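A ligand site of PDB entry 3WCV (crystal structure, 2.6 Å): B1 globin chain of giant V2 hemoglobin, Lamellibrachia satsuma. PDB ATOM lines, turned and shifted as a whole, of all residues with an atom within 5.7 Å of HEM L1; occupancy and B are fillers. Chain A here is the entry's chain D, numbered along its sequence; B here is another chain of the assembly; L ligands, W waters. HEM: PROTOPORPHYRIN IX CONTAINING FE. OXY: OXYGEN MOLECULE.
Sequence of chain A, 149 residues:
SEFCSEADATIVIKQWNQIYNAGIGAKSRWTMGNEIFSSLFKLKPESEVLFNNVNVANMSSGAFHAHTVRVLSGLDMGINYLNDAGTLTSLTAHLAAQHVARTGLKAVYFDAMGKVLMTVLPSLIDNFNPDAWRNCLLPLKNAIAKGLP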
ATOM      1  N   PHE A  37     -26.271 -18.043 -12.029  1.00  0.00           N
ATOM      2  CA  PHE A  37     -25.968 -16.665 -12.400  1.00  0.00           C
ATOM      3  C   PHE A  37     -27.109 -16.001 -13.180  1.00  0.00           C
ATOM      4  O   PHE A  37     -27.444 -14.846 -12.890  1.00  0.00           O
ATOM      5  CB  PHE A  37     -24.645 -16.617 -13.164  1.00  0.00           C
ATOM      6  CG  PHE A  37     -23.445 -16.735 -12.282  1.00  0.00           C
ATOM      7  CD1 PHE A  37     -22.947 -15.615 -11.630  1.00  0.00           C
ATOM      8  CD2 PHE A  37     -22.873 -17.974 -12.010  1.00  0.00           C
ATOM      9  CE1 PHE A  37     -21.887 -15.729 -10.724  1.00  0.00           C
ATOM     10  CE2 PHE A  37     -21.822 -18.095 -11.114  1.00  0.00           C
ATOM     11  CZ  PHE A  37     -21.323 -16.976 -10.461  1.00  0.00           C
ATOM     12  N   LEU A  40     -29.126 -14.695 -10.722  1.00  0.00           N
ATOM     13  CA  LEU A  40     -28.523 -13.594  -9.994  1.00  0.00           C
ATOM     14  C   LEU A  40     -28.669 -12.306 -10.810  1.00  0.00           C
ATOM     15  O   LEU A  40     -28.857 -11.225 -10.259  1.00  0.00           O
ATOM     16  CB  LEU A  40     -27.039 -13.855  -9.740  1.00  0.00           C
ATOM     17  CG  LEU A  40     -26.345 -12.664  -9.056  1.00  0.00           C
ATOM     18  CD1 LEU A  40     -26.864 -12.530  -7.642  1.00  0.00           C
ATOM     19  CD2 LEU A  40     -24.841 -12.853  -9.038  1.00  0.00           C
ATOM     20  N   SER A  47     -25.328  -6.309 -11.687  1.00  0.00           N
ATOM     21  CA  SER A  47     -24.118  -7.090 -11.391  1.00  0.00           C
ATOM     22  C   SER A  47     -23.586  -7.920 -12.547  1.00  0.00           C
ATOM     23  O   SER A  47     -22.444  -8.384 -12.485  1.00  0.00           O
ATOM     24  CB  SER A  47     -24.374  -8.006 -10.197  1.00  0.00           C
ATOM     25  OG  SER A  47     -25.335  -8.995 -10.508  1.00  0.00           O
ATOM     26  N   LEU A  50     -20.113  -7.143 -14.026  1.00  0.00           N
ATOM     27  CA  LEU A  50     -18.916  -7.532 -13.278  1.00  0.00           C
ATOM     28  C   LEU A  50     -18.192  -8.746 -13.864  1.00  0.00           C
ATOM     29  O   LEU A  50     -17.009  -8.952 -13.603  1.00  0.00           O
ATOM     30  CB  LEU A  50     -19.283  -7.821 -11.812  1.00  0.00           C
ATOM     31  CG  LEU A  50     -20.024  -6.738 -11.034  1.00  0.00           C
ATOM     32  CD1 LEU A  50     -20.306  -7.232  -9.624  1.00  0.00           C
ATOM     33  CD2 LEU A  50     -19.205  -5.472 -10.988  1.00  0.00           C
ATOM     34  N   PHE A  51     -18.895  -9.538 -14.656  1.00  0.00           N
ATOM     35  CA  PHE A  51     -18.309 -10.736 -15.252  1.00  0.00           C
ATOM     36  C   PHE A  51     -17.893 -10.586 -16.715  1.00  0.00           C
ATOM     37  O   PHE A  51     -17.604 -11.576 -17.379  1.00  0.00           O
ATOM     38  CB  PHE A  51     -19.282 -11.906 -15.110  1.00  0.00           C
ATOM     39  CG  PHE A  51     -19.678 -12.190 -13.690  1.00  0.00           C
ATOM     40  CD1 PHE A  51     -20.811 -11.608 -13.127  1.00  0.00           C
ATOM     41  CD2 PHE A  51     -18.851 -12.977 -12.880  1.00  0.00           C
ATOM     42  CE1 PHE A  51     -21.129 -11.801 -11.786  1.00  0.00           C
ATOM     43  CE2 PHE A  51     -19.154 -13.169 -11.542  1.00  0.00           C
ATOM     44  CZ  PHE A  51     -20.297 -12.580 -10.997  1.00  0.00           C
ATOM     45  N   ASN A  53     -15.304  -9.814 -17.781  1.00  0.00           N
ATOM     46  CA  ASN A  53     -13.945 -10.331 -17.909  1.00  0.00           C
ATOM     47  C   ASN A  53     -13.848 -11.834 -18.164  1.00  0.00           C
ATOM     48  O   ASN A  53     -12.844 -12.307 -18.698  1.00  0.00           O
ATOM     49  CB  ASN A  53     -13.126  -9.982 -16.679  1.00  0.00           C
ATOM     50  CG  ASN A  53     -11.683  -9.707 -17.010  1.00  0.00           C
ATOM     51  OD1 ASN A  53     -11.356  -8.667 -17.596  1.00  0.00           O
ATOM     52  ND2 ASN A  53     -10.802 -10.632 -16.653  1.00  0.00           N
ATOM     53  N   VAL A  54     -14.878 -12.584 -17.765  1.00  0.00           N
ATOM     54  CA  VAL A  54     -14.920 -14.026 -17.975  1.00  0.00           C
ATOM     55  C   VAL A  54     -15.852 -14.353 -19.141  1.00  0.00           C
ATOM     56  O   VAL A  54     -16.338 -15.476 -19.273  1.00  0.00           O
ATOM     57  CB  VAL A  54     -15.409 -14.789 -16.726  1.00  0.00           C
ATOM     58  CG1 VAL A  54     -14.338 -14.759 -15.657  1.00  0.00           C
ATOM     59  CG2 VAL A  54     -16.686 -14.167 -16.209  1.00  0.00           C
ATOM     60  N   HIS A  67     -15.602 -20.259 -15.317  1.00  0.00           N
ATOM     61  CA  HIS A  67     -15.801 -19.400 -14.167  1.00  0.00           C
ATOM     62  C   HIS A  67     -16.800 -20.045 -13.197  1.00  0.00           C
ATOM     63  O   HIS A  67     -16.526 -20.155 -11.997  1.00  0.00           O
ATOM     64  CB  HIS A  67     -16.309 -18.027 -14.607  1.00  0.00           C
ATOM     65  CG  HIS A  67     -16.746 -17.170 -13.473  1.00  0.00           C
ATOM     66  ND1 HIS A  67     -15.861 -16.676 -12.536  1.00  0.00           N
ATOM     67  CD2 HIS A  67     -17.973 -16.777 -13.060  1.00  0.00           C
ATOM     68  CE1 HIS A  67     -16.518 -16.024 -11.591  1.00  0.00           C
ATOM     69  NE2 HIS A  67     -17.812 -16.068 -11.892  1.00  0.00           N
ATOM     70  N   ARG A  70     -15.375 -22.856 -11.457  1.00  0.00           N
ATOM     71  CA  ARG A  70     -14.524 -22.320 -10.401  1.00  0.00           C
ATOM     72  C   ARG A  70     -15.345 -21.925  -9.172  1.00  0.00           C
ATOM     73  O   ARG A  70     -14.980 -22.208  -8.026  1.00  0.00           O
ATOM     74  CB  ARG A  70     -13.810 -21.099 -10.976  1.00  0.00           C
ATOM     75  CG  ARG A  70     -12.409 -20.859 -10.486  1.00  0.00           C
ATOM     76  CD  ARG A  70     -11.770 -19.792 -11.370  1.00  0.00           C
ATOM     77  NE  ARG A  70     -11.460 -20.314 -12.698  1.00  0.00           N
ATOM     78  CZ  ARG A  70     -11.721 -19.669 -13.823  1.00  0.00           C
ATOM     79  NH1 ARG A  70     -12.303 -18.473 -13.790  1.00  0.00           N
ATOM     80  NH2 ARG A  70     -11.379 -20.216 -14.991  1.00  0.00           N
ATOM     81  N   VAL A  71     -16.459 -21.254  -9.431  1.00  0.00           N
ATOM     82  CA  VAL A  71     -17.343 -20.787  -8.372  1.00  0.00           C
ATOM     83  C   VAL A  71     -17.961 -21.933  -7.564  1.00  0.00           C
ATOM     84  O   VAL A  71     -17.988 -21.903  -6.327  1.00  0.00           O
ATOM     85  CB  VAL A  71     -18.470 -19.894  -8.959  1.00  0.00           C
ATOM     86  CG1 VAL A  71     -19.484 -19.567  -7.890  1.00  0.00           C
ATOM     87  CG2 VAL A  71     -17.863 -18.604  -9.515  1.00  0.00           C
ATOM     88  N   GLY A  74     -15.456 -23.697  -5.413  1.00  0.00           N
ATOM     89  CA  GLY A  74     -15.201 -22.916  -4.212  1.00  0.00           C
ATOM     90  C   GLY A  74     -16.291 -23.207  -3.192  1.00  0.00           C
ATOM     91  O   GLY A  74     -16.028 -23.473  -2.001  1.00  0.00           O
ATOM     92  N   LEU A  75     -17.529 -23.158  -3.667  1.00  0.00           N
ATOM     93  CA  LEU A  75     -18.660 -23.440  -2.820  1.00  0.00           C
ATOM     94  C   LEU A  75     -18.514 -24.849  -2.229  1.00  0.00           C
ATOM     95  O   LEU A  75     -18.776 -25.052  -1.044  1.00  0.00           O
ATOM     96  CB  LEU A  75     -19.949 -23.335  -3.631  1.00  0.00           C
ATOM     97  CG  LEU A  75     -21.246 -23.696  -2.914  1.00  0.00           C
ATOM     98  CD1 LEU A  75     -21.298 -22.978  -1.580  1.00  0.00           C
ATOM     99  CD2 LEU A  75     -22.426 -23.285  -3.785  1.00  0.00           C
ATOM    100  N   LEU A  95     -11.162 -16.337  -0.013  1.00  0.00           N
ATOM    101  CA  LEU A  95     -12.230 -16.112  -0.992  1.00  0.00           C
ATOM    102  C   LEU A  95     -12.710 -14.684  -0.840  1.00  0.00           C
ATOM    103  O   LEU A  95     -13.099 -14.046  -1.818  1.00  0.00           O
ATOM    104  CB  LEU A  95     -13.417 -17.052  -0.742  1.00  0.00           C
ATOM    105  CG  LEU A  95     -13.425 -18.413  -1.422  1.00  0.00           C
ATOM    106  CD1 LEU A  95     -14.483 -19.329  -0.827  1.00  0.00           C
ATOM    107  CD2 LEU A  95     -13.692 -18.177  -2.889  1.00  0.00           C
ATOM    108  N   GLN A  98     -10.493 -12.411  -2.656  1.00  0.00           N
ATOM    109  CA  GLN A  98     -10.680 -12.514  -4.097  1.00  0.00           C
ATOM    110  C   GLN A  98     -11.908 -11.746  -4.568  1.00  0.00           C
ATOM    111  O   GLN A  98     -12.092 -11.531  -5.768  1.00  0.00           O
ATOM    112  CB  GLN A  98     -10.804 -13.975  -4.521  1.00  0.00           C
ATOM    113  CG  GLN A  98      -9.534 -14.810  -4.315  1.00  0.00           C
ATOM    114  CD  GLN A  98      -9.705 -16.274  -4.726  1.00  0.00           C
ATOM    115  OE1 GLN A  98     -10.627 -16.955  -4.259  1.00  0.00           O
ATOM    116  NE2 GLN A  98      -8.813 -16.767  -5.591  1.00  0.00           N
ATOM    117  N   HIS A  99     -12.766 -11.330  -3.637  1.00  0.00           N
ATOM    118  CA  HIS A  99     -13.957 -10.586  -4.009  1.00  0.00           C
ATOM    119  C   HIS A  99     -13.850  -9.107  -3.697  1.00  0.00           C
ATOM    120  O   HIS A  99     -14.460  -8.275  -4.374  1.00  0.00           O
ATOM    121  CB  HIS A  99     -15.197 -11.199  -3.361  1.00  0.00           C
ATOM    122  CG  HIS A  99     -15.684 -12.431  -4.055  1.00  0.00           C
ATOM    123  ND1 HIS A  99     -15.087 -13.670  -3.908  1.00  0.00           N
ATOM    124  CD2 HIS A  99     -16.683 -12.615  -4.962  1.00  0.00           C
ATOM    125  CE1 HIS A  99     -15.679 -14.549  -4.696  1.00  0.00           C
ATOM    126  NE2 HIS A  99     -16.654 -13.936  -5.338  1.00  0.00           N
ATOM    127  N   ARG A 102     -12.212  -6.831  -6.186  1.00  0.00           N
ATOM    128  CA  ARG A 102     -13.101  -6.609  -7.316  1.00  0.00           C
ATOM    129  C   ARG A 102     -14.021  -5.426  -7.051  1.00  0.00           C
ATOM    130  O   ARG A 102     -15.004  -5.542  -6.320  1.00  0.00           O
ATOM    131  CB  ARG A 102     -13.939  -7.870  -7.585  1.00  0.00           C
ATOM    132  CG  ARG A 102     -14.310  -8.041  -9.036  1.00  0.00           C
ATOM    133  CD  ARG A 102     -13.078  -8.337  -9.870  1.00  0.00           C
ATOM    134  NE  ARG A 102     -13.400  -8.637 -11.261  1.00  0.00           N
ATOM    135  CZ  ARG A 102     -12.590  -9.300 -12.090  1.00  0.00           C
ATOM    136  NH1 ARG A 102     -11.417  -9.733 -11.665  1.00  0.00           N
ATOM    137  NH2 ARG A 102     -12.966  -9.531 -13.341  1.00  0.00           N
ATOM    138  N   LEU A 105     -18.462  -4.639  -6.264  1.00  0.00           N
ATOM    139  CA  LEU A 105     -19.148  -5.674  -5.498  1.00  0.00           C
ATOM    140  C   LEU A 105     -19.750  -5.217  -4.184  1.00  0.00           C
ATOM    141  O   LEU A 105     -19.027  -4.835  -3.253  1.00  0.00           O
ATOM    142  CB  LEU A 105     -18.197  -6.841  -5.208  1.00  0.00           C
ATOM    143  CG  LEU A 105     -18.214  -7.963  -6.234  1.00  0.00           C
ATOM    144  CD1 LEU A 105     -17.624  -7.465  -7.548  1.00  0.00           C
ATOM    145  CD2 LEU A 105     -17.408  -9.134  -5.718  1.00  0.00           C
ATOM    146  N   TYR A 109     -25.214  -8.069  -3.139  1.00  0.00           N
ATOM    147  CA  TYR A 109     -25.182  -9.031  -4.230  1.00  0.00           C
ATOM    148  C   TYR A 109     -25.079 -10.454  -3.690  1.00  0.00           C
ATOM    149  O   TYR A 109     -25.557 -11.405  -4.309  1.00  0.00           O
ATOM    150  CB  TYR A 109     -24.006  -8.770  -5.169  1.00  0.00           C
ATOM    151  CG  TYR A 109     -24.052  -7.437  -5.878  1.00  0.00           C
ATOM    152  CD1 TYR A 109     -25.226  -6.973  -6.451  1.00  0.00           C
ATOM    153  CD2 TYR A 109     -22.891  -6.675  -6.013  1.00  0.00           C
ATOM    154  CE1 TYR A 109     -25.260  -5.759  -7.152  1.00  0.00           C
ATOM    155  CE2 TYR A 109     -22.909  -5.475  -6.707  1.00  0.00           C
ATOM    156  CZ  TYR A 109     -24.097  -5.021  -7.281  1.00  0.00           C
ATOM    157  OH  TYR A 109     -24.115  -3.840  -7.981  1.00  0.00           O
ATOM    158  N   PHE A 110     -24.432 -10.585  -2.535  1.00  0.00           N
ATOM    159  CA  PHE A 110     -24.276 -11.884  -1.899  1.00  0.00           C
ATOM    160  C   PHE A 110     -25.552 -12.256  -1.182  1.00  0.00           C
ATOM    161  O   PHE A 110     -25.737 -13.410  -0.789  1.00  0.00           O
ATOM    162  CB  PHE A 110     -23.116 -11.888  -0.917  1.00  0.00           C
ATOM    163  CG  PHE A 110     -21.782 -12.080  -1.572  1.00  0.00           C
ATOM    164  CD1 PHE A 110     -21.224 -11.055  -2.336  1.00  0.00           C
ATOM    165  CD2 PHE A 110     -21.089 -13.273  -1.439  1.00  0.00           C
ATOM    166  CE1 PHE A 110     -19.986 -11.237  -2.956  1.00  0.00           C
ATOM    167  CE2 PHE A 110     -19.851 -13.455  -2.059  1.00  0.00           C
ATOM    168  CZ  PHE A 110     -19.299 -12.441  -2.819  1.00  0.00           C
ATOM    169  N   MET A 113     -27.454 -13.668  -4.157  1.00  0.00           N
ATOM    170  CA  MET A 113     -26.858 -14.978  -4.469  1.00  0.00           C
ATOM    171  C   MET A 113     -27.411 -15.999  -3.476  1.00  0.00           C
ATOM    172  O   MET A 113     -27.680 -17.139  -3.838  1.00  0.00           O
ATOM    173  CB  MET A 113     -25.340 -14.909  -4.338  1.00  0.00           C
ATOM    174  CG  MET A 113     -24.622 -16.239  -4.509  1.00  0.00           C
ATOM    175  SD  MET A 113     -24.725 -16.996  -6.174  1.00  0.00           S
ATOM    176  CE  MET A 113     -23.194 -16.561  -6.841  1.00  0.00           C
ATOM    177  N   LEU A 117     -29.469 -19.398  -4.454  1.00  0.00           N
ATOM    178  CA  LEU A 117     -29.102 -20.726  -4.044  1.00  0.00           C
ATOM    179  C   LEU A 117     -30.275 -21.412  -3.341  1.00  0.00           C
ATOM    180  O   LEU A 117     -30.550 -22.589  -3.602  1.00  0.00           O
ATOM    181  CB  LEU A 117     -27.847 -20.695  -3.134  1.00  0.00           C
ATOM    182  CG  LEU A 117     -26.555 -20.292  -3.880  1.00  0.00           C
ATOM    183  CD1 LEU A 117     -25.366 -20.349  -2.960  1.00  0.00           C
ATOM    184  CD2 LEU A 117     -26.354 -21.210  -5.074  1.00  0.00           C
ATOM    185  N   LYS A 141     -21.489 -16.886   3.791  1.00  0.00           N
ATOM    186  CA  LYS A 141     -21.736 -15.718   2.987  1.00  0.00           C
ATOM    187  C   LYS A 141     -21.234 -14.464   3.648  1.00  0.00           C
ATOM    188  O   LYS A 141     -20.609 -13.630   3.002  1.00  0.00           O
ATOM    189  CB  LYS A 141     -23.225 -15.641   2.653  1.00  0.00           C
ATOM    190  CG  LYS A 141     -23.598 -14.488   1.719  1.00  0.00           C
ATOM    191  CD  LYS A 141     -24.029 -13.261   2.498  1.00  0.00           C
ATOM    192  CE  LYS A 141     -25.359 -13.514   3.213  1.00  0.00           C
ATOM    193  NZ  LYS A 141     -25.787 -12.335   4.004  1.00  0.00           N
ATOM    194  N   ILE A 144     -17.533 -14.232   3.343  1.00  0.00           N
ATOM    195  CA  ILE A 144     -17.062 -13.934   1.999  1.00  0.00           C
ATOM    196  C   ILE A 144     -17.510 -12.553   1.531  1.00  0.00           C
ATOM    197  O   ILE A 144     -16.964 -12.018   0.563  1.00  0.00           O
ATOM    198  CB  ILE A 144     -17.574 -14.977   0.981  1.00  0.00           C
ATOM    199  CG1 ILE A 144     -17.195 -16.381   1.454  1.00  0.00           C
ATOM    200  CG2 ILE A 144     -16.962 -14.717  -0.383  1.00  0.00           C
ATOM    201  CD1 ILE A 144     -17.750 -17.480   0.567  1.00  0.00           C
ATOM    202  N   ARG B  72     -11.572 -29.705 -10.162  1.00  0.00           N
ATOM    203  CA  ARG B  72     -12.368 -28.978 -11.165  1.00  0.00           C
ATOM    204  C   ARG B  72     -11.723 -29.115 -12.546  1.00  0.00           C
ATOM    205  O   ARG B  72     -12.422 -29.167 -13.569  1.00  0.00           O
ATOM    206  CB  ARG B  72     -12.482 -27.516 -10.793  1.00  0.00           C
ATOM    207  CG  ARG B  72     -11.191 -26.768 -10.924  1.00  0.00           C
ATOM    208  CD  ARG B  72     -11.355 -25.387 -10.383  1.00  0.00           C
ATOM    209  NE  ARG B  72     -10.478 -24.471 -11.094  1.00  0.00           N
ATOM    210  CZ  ARG B  72      -9.814 -23.487 -10.516  1.00  0.00           C
ATOM    211  NH1 ARG B  72      -9.960 -23.294  -9.224  1.00  0.00           N
ATOM    212  NH2 ARG B  72      -9.016 -22.729 -11.224  1.00  0.00           N
ATOM    213  N   HIS B  89      -6.404 -19.634 -16.614  1.00  0.00           N
ATOM    214  CA  HIS B  89      -6.673 -18.950 -15.356  1.00  0.00           C
ATOM    215  C   HIS B  89      -5.605 -19.354 -14.319  1.00  0.00           C
ATOM    216  O   HIS B  89      -4.938 -18.518 -13.711  1.00  0.00           O
ATOM    217  CB  HIS B  89      -8.073 -19.337 -14.859  1.00  0.00           C
ATOM    218  CG  HIS B  89      -8.536 -18.549 -13.677  1.00  0.00           C
ATOM    219  ND1 HIS B  89      -9.122 -17.308 -13.802  1.00  0.00           N
ATOM    220  CD2 HIS B  89      -8.461 -18.797 -12.350  1.00  0.00           C
ATOM    221  CE1 HIS B  89      -9.400 -16.825 -12.606  1.00  0.00           C
ATOM    222  NE2 HIS B  89      -8.999 -17.712 -11.704  1.00  0.00           N
ATOM    223  N   GLN B  93      -2.174 -17.274 -12.550  1.00  0.00           N
ATOM    224  CA  GLN B  93      -1.949 -17.224 -11.111  1.00  0.00           C
ATOM    225  C   GLN B  93      -0.588 -17.782 -10.700  1.00  0.00           C
ATOM    226  O   GLN B  93      -0.073 -17.432  -9.641  1.00  0.00           O
ATOM    227  CB  GLN B  93      -3.033 -17.994 -10.354  1.00  0.00           C
ATOM    228  CG  GLN B  93      -4.432 -17.417 -10.486  1.00  0.00           C
ATOM    229  CD  GLN B  93      -5.474 -18.299  -9.866  1.00  0.00           C
ATOM    230  OE1 GLN B  93      -5.621 -19.461 -10.233  1.00  0.00           O
ATOM    231  NE2 GLN B  93      -6.229 -17.749  -8.927  1.00  0.00           N
HETATM  232  CHA HEM L   1     -14.666 -14.887  -8.735  1.00  0.00           C
HETATM  233  CHB HEM L   1     -16.568 -17.960  -5.660  1.00  0.00           C
HETATM  234  CHC HEM L   1     -20.471 -15.145  -5.142  1.00  0.00           C
HETATM  235  CHD HEM L   1     -18.464 -12.000  -8.215  1.00  0.00           C
HETATM  236  C1A HEM L   1     -14.830 -15.983  -7.938  1.00  0.00           C
HETATM  237  C2A HEM L   1     -13.909 -17.031  -7.866  1.00  0.00           C
HETATM  238  C3A HEM L   1     -14.428 -17.904  -6.993  1.00  0.00           C
HETATM  239  C4A HEM L   1     -15.714 -17.393  -6.522  1.00  0.00           C
HETATM  240  CMA HEM L   1     -13.799 -19.227  -6.548  1.00  0.00           C
HETATM  241  CAA HEM L   1     -12.603 -17.172  -8.604  1.00  0.00           C
HETATM  242  CBA HEM L   1     -11.438 -16.597  -7.880  1.00  0.00           C
HETATM  243  CGA HEM L   1     -10.128 -16.731  -8.638  1.00  0.00           C
HETATM  244  O1A HEM L   1      -9.548 -15.701  -9.056  1.00  0.00           O
HETATM  245  O2A HEM L   1      -9.707 -17.840  -8.820  1.00  0.00           O
HETATM  246  C1B HEM L   1     -17.830 -17.491  -5.223  1.00  0.00           C
HETATM  247  C2B HEM L   1     -18.711 -18.219  -4.294  1.00  0.00           C
HETATM  248  C3B HEM L   1     -19.874 -17.377  -4.164  1.00  0.00           C
HETATM  249  C4B HEM L   1     -19.599 -16.235  -4.978  1.00  0.00           C
HETATM  250  CMB HEM L   1     -18.455 -19.528  -3.662  1.00  0.00           C
HETATM  251  CAB HEM L   1     -21.033 -17.717  -3.333  1.00  0.00           C
HETATM  252  CBB HEM L   1     -21.174 -17.378  -2.066  1.00  0.00           C
HETATM  253  C1C HEM L   1     -20.237 -14.028  -5.943  1.00  0.00           C
HETATM  254  C2C HEM L   1     -21.208 -12.916  -6.045  1.00  0.00           C
HETATM  255  C3C HEM L   1     -20.667 -11.971  -6.941  1.00  0.00           C
HETATM  256  C4C HEM L   1     -19.330 -12.582  -7.342  1.00  0.00           C
HETATM  257  CMC HEM L   1     -22.555 -12.857  -5.314  1.00  0.00           C
HETATM  258  CAC HEM L   1     -21.211 -10.787  -7.328  1.00  0.00           C
HETATM  259  CBC HEM L   1     -21.867 -10.300  -8.317  1.00  0.00           C
HETATM  260  C1D HEM L   1     -17.241 -12.518  -8.634  1.00  0.00           C
HETATM  261  C2D HEM L   1     -16.320 -11.828  -9.636  1.00  0.00           C
HETATM  262  C3D HEM L   1     -15.251 -12.676  -9.775  1.00  0.00           C
HETATM  263  C4D HEM L   1     -15.506 -13.825  -8.883  1.00  0.00           C
HETATM  264  CMD HEM L   1     -16.609 -10.497 -10.300  1.00  0.00           C
HETATM  265  CAD HEM L   1     -14.029 -12.487 -10.663  1.00  0.00           C
HETATM  266  CBD HEM L   1     -14.304 -12.983 -12.070  1.00  0.00           C
HETATM  267  CGD HEM L   1     -13.174 -12.868 -13.015  1.00  0.00           C
HETATM  268  O1D HEM L   1     -12.186 -13.653 -12.906  1.00  0.00           O
HETATM  269  O2D HEM L   1     -13.224 -12.036 -13.926  1.00  0.00           O
HETATM  270  NA  HEM L   1     -15.955 -16.190  -7.125  1.00  0.00           N
HETATM  271  NB  HEM L   1     -18.342 -16.326  -5.645  1.00  0.00           N
HETATM  272  NC  HEM L   1     -19.126 -13.775  -6.737  1.00  0.00           N
HETATM  273  ND  HEM L   1     -16.703 -13.696  -8.236  1.00  0.00           N
HETATM  274 FE   HEM L   1     -17.527 -14.978  -6.913  1.00  0.00          FE
HETATM  275  O1  OXY L   2     -18.303 -15.889  -8.236  1.00  0.00           O
HETATM  276  O2  OXY L   2     -18.854 -15.400  -9.234  1.00  0.00           O
HETATM  277  CHA HEM L   3      -1.625 -21.456  -5.542  1.00  0.00           C
HETATM  278  CHB HEM L   3      -3.356 -25.028  -8.084  1.00  0.00           C
HETATM  279  CHC HEM L   3       1.021 -26.740  -8.802  1.00  0.00           C
HETATM  280  CHD HEM L   3       2.776 -23.120  -6.277  1.00  0.00           C
HETATM  281  C1A HEM L   3      -2.546 -22.270  -6.169  1.00  0.00           C
HETATM  282  C2A HEM L   3      -3.941 -22.063  -6.123  1.00  0.00           C
HETATM  283  C3A HEM L   3      -4.441 -23.070  -6.856  1.00  0.00           C
HETATM  284  C4A HEM L   3      -3.322 -23.905  -7.333  1.00  0.00           C
HETATM  285  CMA HEM L   3      -5.897 -23.378  -7.150  1.00  0.00           C
HETATM  286  CAA HEM L   3      -4.707 -20.966  -5.412  1.00  0.00           C
HETATM  287  CBA HEM L   3      -5.000 -19.783  -6.288  1.00  0.00           C
HETATM  288  CGA HEM L   3      -5.790 -18.670  -5.591  1.00  0.00           C
HETATM  289  O1A HEM L   3      -5.232 -17.575  -5.321  1.00  0.00           O
HETATM  290  O2A HEM L   3      -6.935 -18.889  -5.311  1.00  0.00           O
HETATM  291  C1B HEM L   3      -2.321 -25.876  -8.551  1.00  0.00           C
HETATM  292  C2B HEM L   3      -2.522 -27.088  -9.345  1.00  0.00           C
HETATM  293  C3B HEM L   3      -1.204 -27.578  -9.548  1.00  0.00           C
HETATM  294  C4B HEM L   3      -0.373 -26.651  -8.874  1.00  0.00           C
HETATM  295  CMB HEM L   3      -3.812 -27.643  -9.791  1.00  0.00           C
HETATM  296  CAB HEM L   3      -0.896 -28.776 -10.282  1.00  0.00           C
HETATM  297  CBB HEM L   3      -0.807 -28.855 -11.592  1.00  0.00           C
HETATM  298  C1C HEM L   3       1.884 -25.886  -8.166  1.00  0.00           C
HETATM  299  C2C HEM L   3       3.360 -26.123  -8.160  1.00  0.00           C
HETATM  300  C3C HEM L   3       3.914 -25.082  -7.438  1.00  0.00           C
HETATM  301  C4C HEM L   3       2.684 -24.250  -7.036  1.00  0.00           C
HETATM  302  CMC HEM L   3       4.077 -27.316  -8.836  1.00  0.00           C
HETATM  303  CAC HEM L   3       5.222 -24.875  -7.149  1.00  0.00           C
HETATM  304  CBC HEM L   3       6.129 -25.432  -6.423  1.00  0.00           C
HETATM  305  C1D HEM L   3       1.724 -22.315  -5.837  1.00  0.00           C
HETATM  306  C2D HEM L   3       1.929 -21.058  -4.960  1.00  0.00           C
HETATM  307  C3D HEM L   3       0.646 -20.608  -4.769  1.00  0.00           C
HETATM  308  C4D HEM L   3      -0.264 -21.565  -5.502  1.00  0.00           C
HETATM  309  CMD HEM L   3       3.263 -20.524  -4.460  1.00  0.00           C
HETATM  310  CAD HEM L   3       0.203 -19.395  -3.978  1.00  0.00           C
HETATM  311  CBD HEM L   3      -0.105 -19.713  -2.554  1.00  0.00           C
HETATM  312  CGD HEM L   3      -0.573 -18.535  -1.847  1.00  0.00           C
HETATM  313  O1D HEM L   3       0.227 -17.886  -1.107  1.00  0.00           O
HETATM  314  O2D HEM L   3      -1.776 -18.184  -2.008  1.00  0.00           O
HETATM  315  NA  HEM L   3      -2.169 -23.395  -6.903  1.00  0.00           N
HETATM  316  NB  HEM L   3      -1.074 -25.610  -8.277  1.00  0.00           N
HETATM  317  NC  HEM L   3       1.543 -24.764  -7.484  1.00  0.00           N
HETATM  318  ND  HEM L   3       0.434 -22.549  -6.109  1.00  0.00           N
HETATM  319 FE   HEM L   3      -0.316 -24.068  -7.212  1.00  0.00          FE
HETATM  320  O   HOH W   1     -13.170 -16.142 -12.002  1.00  0.00           O
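A ring nitrogen (ND1) of His 99 lies within hydrogen-bond range of the backbone carbonyl oxygen of Leu 95, at 2.9 Å.
A ring nitrogen (ND1) of His 89 of chain B lies within hydrogen-bond range of the guanidinium group (NH1) of Arg 70 (3.4 Å).
An oxygen (O1) of OXY L2 is bound to an iron atom (FE) of HEM L1 (1.8 Å).
A ring nitrogen (NE2) of His 99 binds an iron atom (FE) of HEM L1.
An oxygen (O2D) of HEM L1 lies within salt-bridge range of the guanidinium group (NH2) of Arg 102.
A ring nitrogen (NE2) of His 89 of chain B is in hydrogen-bond range of an oxygen (O2A) of HEM L1, at 3.0 Å.
An oxygen (O2A) of HEM L1 sits at hydrogen-bond distance from the side-chain amide nitrogen (NE2) of Gln 93 of chain B, 3.5 Å away.
NE2 of His 67 lies within hydrogen-bond range of O2 of OXY L2, at 2.9 Å.
O2A of HEM L3 sits at hydrogen-bond distance from NE2 of Gln 98 (2.8 Å).
Water W1 lies within hydrogen-bond range of ND1 of His 67 (2.8 Å), O1D of HEM L1 (2.8 Å) and NH1 of Arg 70 (3.1 Å).
Leu 40 touches HEM L1 (CD2 to CBC, 3.99 Å).
CB of Ser 47 touches CBC of HEM L1 (3.9 Å).
Leu 50 touches HEM L1.
Phe 51 touches HEM L1 (CZ to CHD, 3.4 Å).
CB of Asn 53 touches O2D of HEM L1 (3.4 Å).
Val 54 touches HEM L1.
His 67 touches HEM L1.
Arg 70 touches HEM L1.
O of Val 71 touches CMB of HEM L1, at 3.6 Å.
Leu 75 touches HEM L1 (N to CMB, 3.7 Å).
CD2 of Leu 95 touches CMA of HEM L1, at 3.8 Å.
Gln 98 touches HEM L1.
CD2 of Leu 105 touches CHD of HEM L1 (3.9 Å).
Tyr 109 touches HEM L1.
Phe 110 touches HEM L1 (CE2 to CHC, 3.6 Å).
CE of Met 113 touches CHC of HEM L1, at 3.5 Å.
Hydrophobic or aromatic side chains that line HEM L1: Leu 40, Leu 50, Phe 51, Val 54, His 67, Val 71, Leu 95, His 99, Leu 105, Phe 110, Met 113 and His 89 of chain B.
Of the 26 residues printed, 20 come within 4 Å of HEM L1.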
